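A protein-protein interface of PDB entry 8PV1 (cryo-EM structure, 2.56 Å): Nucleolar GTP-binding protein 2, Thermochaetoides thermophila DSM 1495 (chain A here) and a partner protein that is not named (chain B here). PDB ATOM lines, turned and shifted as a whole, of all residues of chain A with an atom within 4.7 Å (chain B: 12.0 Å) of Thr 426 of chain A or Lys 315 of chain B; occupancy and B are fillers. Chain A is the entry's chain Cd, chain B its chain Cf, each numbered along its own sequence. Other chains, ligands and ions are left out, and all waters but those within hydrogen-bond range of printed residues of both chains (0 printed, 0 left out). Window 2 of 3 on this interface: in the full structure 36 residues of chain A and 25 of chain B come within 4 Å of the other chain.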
ATOM      1  N   HIS A 422     -23.927   9.036  25.887  1.00  0.00           N
ATOM      2  CA  HIS A 422     -24.709   7.814  25.719  1.00  0.00           C
ATOM      3  C   HIS A 422     -25.888   8.035  24.775  1.00  0.00           C
ATOM      4  O   HIS A 422     -26.152   7.206  23.897  1.00  0.00           O
ATOM      5  CB  HIS A 422     -25.182   7.305  27.080  1.00  0.00           C
ATOM      6  CG  HIS A 422     -24.092   6.698  27.906  1.00  0.00           C
ATOM      7  ND1 HIS A 422     -24.006   6.870  29.270  1.00  0.00           N
ATOM      8  CD2 HIS A 422     -23.034   5.928  27.557  1.00  0.00           C
ATOM      9  CE1 HIS A 422     -22.946   6.227  29.727  1.00  0.00           C
ATOM     10  NE2 HIS A 422     -22.338   5.648  28.708  1.00  0.00           N
ATOM     11  N   MET A 423     -26.596   9.159  24.927  1.00  0.00           N
ATOM     12  CA  MET A 423     -27.683   9.500  24.009  1.00  0.00           C
ATOM     13  C   MET A 423     -27.165   9.712  22.592  1.00  0.00           C
ATOM     14  O   MET A 423     -27.773   9.249  21.616  1.00  0.00           O
ATOM     15  CB  MET A 423     -28.409  10.756  24.492  1.00  0.00           C
ATOM     16  CG  MET A 423     -29.153  10.609  25.802  1.00  0.00           C
ATOM     17  SD  MET A 423     -30.457   9.369  25.746  1.00  0.00           S
ATOM     18  CE  MET A 423     -31.638  10.156  24.664  1.00  0.00           C
ATOM     19  N   GLU A 424     -26.039  10.423  22.466  1.00  0.00           N
ATOM     20  CA  GLU A 424     -25.464  10.695  21.153  1.00  0.00           C
ATOM     21  C   GLU A 424     -25.025   9.413  20.462  1.00  0.00           C
ATOM     22  O   GLU A 424     -25.244   9.241  19.259  1.00  0.00           O
ATOM     23  CB  GLU A 424     -24.289  11.660  21.288  1.00  0.00           C
ATOM     24  CG  GLU A 424     -24.685  13.055  21.721  1.00  0.00           C
ATOM     25  CD  GLU A 424     -23.501  13.887  22.164  1.00  0.00           C
ATOM     26  OE1 GLU A 424     -22.413  13.311  22.368  1.00  0.00           O
ATOM     27  OE2 GLU A 424     -23.661  15.116  22.313  1.00  0.00           O
ATOM     28  N   ARG A 425     -24.423   8.490  21.212  1.00  0.00           N
ATOM     29  CA  ARG A 425     -23.955   7.245  20.622  1.00  0.00           C
ATOM     30  C   ARG A 425     -25.117   6.303  20.336  1.00  0.00           C
ATOM     31  O   ARG A 425     -25.048   5.484  19.412  1.00  0.00           O
ATOM     32  CB  ARG A 425     -22.937   6.600  21.560  1.00  0.00           C
ATOM     33  CG  ARG A 425     -22.130   5.477  20.964  1.00  0.00           C
ATOM     34  CD  ARG A 425     -20.677   5.629  21.380  1.00  0.00           C
ATOM     35  NE  ARG A 425     -20.473   5.277  22.780  1.00  0.00           N
ATOM     36  CZ  ARG A 425     -19.839   6.041  23.660  1.00  0.00           C
ATOM     37  NH1 ARG A 425     -19.330   7.213  23.316  1.00  0.00           N
ATOM     38  NH2 ARG A 425     -19.714   5.618  24.913  1.00  0.00           N
ATOM     39  N   THR A 426     -26.198   6.408  21.115  1.00  0.00           N
ATOM     40  CA  THR A 426     -27.372   5.577  20.876  1.00  0.00           C
ATOM     41  C   THR A 426     -28.108   6.000  19.614  1.00  0.00           C
ATOM     42  O   THR A 426     -28.469   5.157  18.786  1.00  0.00           O
ATOM     43  CB  THR A 426     -28.309   5.645  22.083  1.00  0.00           C
ATOM     44  OG1 THR A 426     -27.609   5.229  23.260  1.00  0.00           O
ATOM     45  CG2 THR A 426     -29.520   4.747  21.877  1.00  0.00           C
ATOM     46  N   TYR A 427     -28.340   7.302  19.442  1.00  0.00           N
ATOM     47  CA  TYR A 427     -29.184   7.774  18.351  1.00  0.00           C
ATOM     48  C   TYR A 427     -28.402   8.356  17.179  1.00  0.00           C
ATOM     49  O   TYR A 427     -29.026   8.814  16.215  1.00  0.00           O
ATOM     50  CB  TYR A 427     -30.196   8.792  18.875  1.00  0.00           C
ATOM     51  CG  TYR A 427     -31.281   8.151  19.705  1.00  0.00           C
ATOM     52  CD1 TYR A 427     -32.214   7.306  19.119  1.00  0.00           C
ATOM     53  CD2 TYR A 427     -31.369   8.378  21.071  1.00  0.00           C
ATOM     54  CE1 TYR A 427     -33.204   6.710  19.867  1.00  0.00           C
ATOM     55  CE2 TYR A 427     -32.361   7.785  21.830  1.00  0.00           C
ATOM     56  CZ  TYR A 427     -33.274   6.951  21.221  1.00  0.00           C
ATOM     57  OH  TYR A 427     -34.263   6.358  21.966  1.00  0.00           O
ATOM     58  N   GLU A 428     -27.064   8.314  17.226  1.00  0.00           N
ATOM     59  CA  GLU A 428     -26.181   8.802  16.159  1.00  0.00           C
ATOM     60  C   GLU A 428     -26.486  10.254  15.793  1.00  0.00           C
ATOM     61  O   GLU A 428     -26.575  10.626  14.622  1.00  0.00           O
ATOM     62  CB  GLU A 428     -26.246   7.896  14.928  1.00  0.00           C
ATOM     63  CG  GLU A 428     -26.096   6.420  15.245  1.00  0.00           C
ATOM     64  CD  GLU A 428     -25.765   5.592  14.021  1.00  0.00           C
ATOM     65  OE1 GLU A 428     -26.426   5.783  12.977  1.00  0.00           O
ATOM     66  OE2 GLU A 428     -24.844   4.754  14.100  1.00  0.00           O
ATOM     67  N   LYS A 472     -32.740  -0.065  26.391  1.00  0.00           N
ATOM     68  CA  LYS A 472     -32.092   0.237  25.126  1.00  0.00           C
ATOM     69  C   LYS A 472     -31.191   1.459  25.188  1.00  0.00           C
ATOM     70  O   LYS A 472     -30.396   1.666  24.267  1.00  0.00           O
ATOM     71  CB  LYS A 472     -33.143   0.433  24.024  1.00  0.00           C
ATOM     72  CG  LYS A 472     -33.901  -0.840  23.694  1.00  0.00           C
ATOM     73  CD  LYS A 472     -34.815  -0.652  22.503  1.00  0.00           C
ATOM     74  CE  LYS A 472     -35.416  -1.970  22.056  1.00  0.00           C
ATOM     75  NZ  LYS A 472     -36.126  -2.656  23.166  1.00  0.00           N
ATOM     76  N   ILE A 473     -31.292   2.264  26.240  1.00  0.00           N
ATOM     77  CA  ILE A 473     -30.378   3.367  26.494  1.00  0.00           C
ATOM     78  C   ILE A 473     -29.672   3.083  27.813  1.00  0.00           C
ATOM     79  O   ILE A 473     -30.337   2.762  28.799  1.00  0.00           O
ATOM     80  CB  ILE A 473     -31.093   4.729  26.554  1.00  0.00           C
ATOM     81  CG1 ILE A 473     -32.091   4.863  25.404  1.00  0.00           C
ATOM     82  CG2 ILE A 473     -30.081   5.849  26.504  1.00  0.00           C
ATOM     83  CD1 ILE A 473     -33.047   6.025  25.556  1.00  0.00           C
ATOM     84  N   PRO A 474     -28.343   3.168  27.876  1.00  0.00           N
ATOM     85  CA  PRO A 474     -27.643   2.892  29.138  1.00  0.00           C
ATOM     86  C   PRO A 474     -27.867   3.997  30.162  1.00  0.00           C
ATOM     87  O   PRO A 474     -27.612   5.173  29.897  1.00  0.00           O
ATOM     88  CB  PRO A 474     -26.171   2.806  28.717  1.00  0.00           C
ATOM     89  CG  PRO A 474     -26.098   3.546  27.428  1.00  0.00           C
ATOM     90  CD  PRO A 474     -27.408   3.327  26.749  1.00  0.00           C
ATOM     91  N   THR B 311     -22.424  -8.079  30.829  1.00  0.00           N
ATOM     92  CA  THR B 311     -23.464  -7.070  30.733  1.00  0.00           C
ATOM     93  C   THR B 311     -23.966  -6.968  29.296  1.00  0.00           C
ATOM     94  O   THR B 311     -23.336  -7.452  28.352  1.00  0.00           O
ATOM     95  CB  THR B 311     -22.949  -5.715  31.215  1.00  0.00           C
ATOM     96  OG1 THR B 311     -21.700  -5.418  30.580  1.00  0.00           O
ATOM     97  CG2 THR B 311     -22.752  -5.737  32.716  1.00  0.00           C
ATOM     98  N   ARG B 312     -25.130  -6.342  29.139  1.00  0.00           N
ATOM     99  CA  ARG B 312     -25.737  -6.222  27.820  1.00  0.00           C
ATOM    100  C   ARG B 312     -24.947  -5.250  26.958  1.00  0.00           C
ATOM    101  O   ARG B 312     -24.690  -4.111  27.357  1.00  0.00           O
ATOM    102  CB  ARG B 312     -27.187  -5.762  27.948  1.00  0.00           C
ATOM    103  CG  ARG B 312     -27.945  -5.741  26.634  1.00  0.00           C
ATOM    104  CD  ARG B 312     -29.440  -5.634  26.865  1.00  0.00           C
ATOM    105  NE  ARG B 312     -30.196  -5.700  25.621  1.00  0.00           N
ATOM    106  CZ  ARG B 312     -30.610  -6.823  25.050  1.00  0.00           C
ATOM    107  NH1 ARG B 312     -30.350  -8.006  25.583  1.00  0.00           N
ATOM    108  NH2 ARG B 312     -31.306  -6.759  23.920  1.00  0.00           N
ATOM    109  N   LYS B 313     -24.565  -5.702  25.762  1.00  0.00           N
ATOM    110  CA  LYS B 313     -23.776  -4.885  24.841  1.00  0.00           C
ATOM    111  C   LYS B 313     -24.711  -3.912  24.125  1.00  0.00           C
ATOM    112  O   LYS B 313     -25.122  -4.104  22.979  1.00  0.00           O
ATOM    113  CB  LYS B 313     -23.012  -5.761  23.858  1.00  0.00           C
ATOM    114  CG  LYS B 313     -22.263  -6.927  24.486  1.00  0.00           C
ATOM    115  CD  LYS B 313     -21.334  -6.482  25.602  1.00  0.00           C
ATOM    116  CE  LYS B 313     -20.721  -7.678  26.308  1.00  0.00           C
ATOM    117  NZ  LYS B 313     -20.120  -7.299  27.612  1.00  0.00           N
ATOM    118  N   MET B 314     -25.051  -2.846  24.841  1.00  0.00           N
ATOM    119  CA  MET B 314     -25.991  -1.861  24.333  1.00  0.00           C
ATOM    120  C   MET B 314     -25.347  -0.999  23.255  1.00  0.00           C
ATOM    121  O   MET B 314     -24.123  -0.910  23.146  1.00  0.00           O
ATOM    122  CB  MET B 314     -26.506  -0.988  25.476  1.00  0.00           C
ATOM    123  CG  MET B 314     -27.473  -1.711  26.393  1.00  0.00           C
ATOM    124  SD  MET B 314     -28.532  -0.609  27.342  1.00  0.00           S
ATOM    125  CE  MET B 314     -27.864  -0.863  28.984  1.00  0.00           C
ATOM    126  N   LYS B 315     -26.200  -0.365  22.447  1.00  0.00           N
ATOM    127  CA  LYS B 315     -25.718   0.453  21.338  1.00  0.00           C
ATOM    128  C   LYS B 315     -25.021   1.713  21.839  1.00  0.00           C
ATOM    129  O   LYS B 315     -24.089   2.212  21.202  1.00  0.00           O
ATOM    130  CB  LYS B 315     -26.886   0.808  20.418  1.00  0.00           C
ATOM    131  CG  LYS B 315     -26.493   1.484  19.119  1.00  0.00           C
ATOM    132  CD  LYS B 315     -27.721   1.934  18.351  1.00  0.00           C
ATOM    133  CE  LYS B 315     -27.362   2.377  16.948  1.00  0.00           C
ATOM    134  NZ  LYS B 315     -28.536   2.951  16.238  1.00  0.00           N
ATOM    135  N   GLY B 316     -25.453   2.234  22.989  1.00  0.00           N
ATOM    136  CA  GLY B 316     -24.848   3.434  23.537  1.00  0.00           C
ATOM    137  C   GLY B 316     -23.524   3.203  24.232  1.00  0.00           C
ATOM    138  O   GLY B 316     -22.879   4.171  24.648  1.00  0.00           O
ATOM    139  N   LEU B 317     -23.104   1.948  24.372  1.00  0.00           N
ATOM    140  CA  LEU B 317     -21.831   1.614  24.989  1.00  0.00           C
ATOM    141  C   LEU B 317     -20.790   1.140  23.985  1.00  0.00           C
ATOM    142  O   LEU B 317     -19.692   0.750  24.391  1.00  0.00           O
ATOM    143  CB  LEU B 317     -22.028   0.538  26.062  1.00  0.00           C
ATOM    144  CG  LEU B 317     -22.911   0.889  27.260  1.00  0.00           C
ATOM    145  CD1 LEU B 317     -23.009  -0.298  28.200  1.00  0.00           C
ATOM    146  CD2 LEU B 317     -22.388   2.112  27.989  1.00  0.00           C
ATOM    147  N   LYS B 318     -21.102   1.162  22.692  1.00  0.00           N
ATOM    148  CA  LYS B 318     -20.187   0.710  21.651  1.00  0.00           C
ATOM    149  C   LYS B 318     -19.547   1.924  20.993  1.00  0.00           C
ATOM    150  O   LYS B 318     -20.215   2.656  20.256  1.00  0.00           O
ATOM    151  CB  LYS B 318     -20.916  -0.140  20.611  1.00  0.00           C
ATOM    152  CG  LYS B 318     -21.507  -1.424  21.160  1.00  0.00           C
ATOM    153  CD  LYS B 318     -22.289  -2.166  20.091  1.00  0.00           C
ATOM    154  CE  LYS B 318     -22.773  -3.514  20.597  1.00  0.00           C
ATOM    155  NZ  LYS B 318     -23.603  -4.219  19.586  1.00  0.00           N
ATOM    156  N   ARG B 319     -18.256   2.121  21.248  1.00  0.00           N
ATOM    157  CA  ARG B 319     -17.517   3.279  20.744  1.00  0.00           C
ATOM    158  C   ARG B 319     -17.427   3.278  19.218  1.00  0.00           C
ATOM    159  O   ARG B 319     -17.084   2.266  18.609  1.00  0.00           O
ATOM    160  CB  ARG B 319     -16.101   3.329  21.337  1.00  0.00           C
ATOM    161  CG  ARG B 319     -15.977   3.872  22.768  1.00  0.00           C
ATOM    162  CD  ARG B 319     -16.447   2.890  23.836  1.00  0.00           C
ATOM    163  NE  ARG B 319     -16.264   3.414  25.185  1.00  0.00           N
ATOM    164  CZ  ARG B 319     -15.153   3.277  25.897  1.00  0.00           C
ATOM    165  NH1 ARG B 319     -14.103   2.627  25.423  1.00  0.00           N
ATOM    166  NH2 ARG B 319     -15.095   3.806  27.116  1.00  0.00           N
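The backbone carbonyl oxygen (O) of Thr 426 of chain A sits close to the side-chain amino group (NZ) of Lys 315 of chain B (3.4 Å).
The guanidinium group (NE) of Arg 425 of chain A sits at hydrogen-bond distance from the backbone carbonyl oxygen (O) of Gly 316 of chain B (3.2 Å).
OG1 of Thr 426 of chain A lies within hydrogen-bond range of O of His 422 of chain A.
Among the printed residues, pairs that only touch across the chains: His 422 of chain A with Gly 316 of chain B (3.4 Å), His 422 of chain A with Leu 317 of chain B (3.6 Å), Arg 425 of chain A with Lys 315 of chain B (3.8 Å), Arg 425 of chain A with Lys 318 of chain B (3.2 Å), Arg 425 of chain A with Arg 319 of chain B (3.99 Å), Thr 426 of chain A with Gly 316 of chain B (3.3 Å), Lys 472 of chain A with Met 314 of chain B (3.998 Å), Ile 473 of chain A with Met 314 of chain B (3.9 Å), Pro 474 of chain A with Met 314 of chain B (3.8 Å) and Pro 474 of chain A with Leu 317 of chain B (3.9 Å).
Of chain B, only Lys 315 (3.3 Å) and Gly 316 (3.3 Å) come within 4 Å of Thr 426 of chain A.
Met 423 of chain A touches none of the printed residues of chain B.
No residue of chain B comes within 4 Å of Tyr 427 of chain A.
No residue of chain B comes within 4 Å of Glu 428 of chain A.
Ile 473 of chain A touches just one residue of chain B: Met 314.
Pro 474 of chain A touches just these residues of chain B: Met 314 (3.8 Å) and Leu 317 (3.9 Å).
Printed residues of chain B within 4 Å of Lys 472 of chain A: Met 314 (3.998 Å).
Of the printed residues of chain A, Lys 318 of chain B touches Arg 425.
Printed residues of chain B within 4 Å of Arg 425 of chain A: Lys 315 (3.8 Å), Gly 316 (3.2 Å), Lys 318 (3.2 Å) and Arg 319 (3.99 Å).
Of the printed residues of chain A, Gly 316 of chain B touches His 422, Arg 425 and Thr 426.
Printed residues of chain B within 4 Å of His 422 of chain A: Gly 316 and Leu 317.
Arg 312 of chain B touches none of the printed residues of chain A.
The nearest residue of chain A that does not touch Lys 315 of chain B is Glu 428 of chain A (4.4 Å).
The nearest printed residue of chain B that does not touch Lys 472 of chain A is Lys 315 of chain B (5.0 Å).
Of the 10 printed residues of chain A, 6 touch a printed residue of chain B.
Of the 9 printed residues of chain B, 6 touch a printed residue of chain A.
Hydrophobic or aromatic side chains of chain B that line the printed part of chain A: Met 314 and Leu 317.
Among the printed residues, no Asp or Glu carboxylate lies within 4 Å of a Lys or Arg side-chain nitrogen of the other chain.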
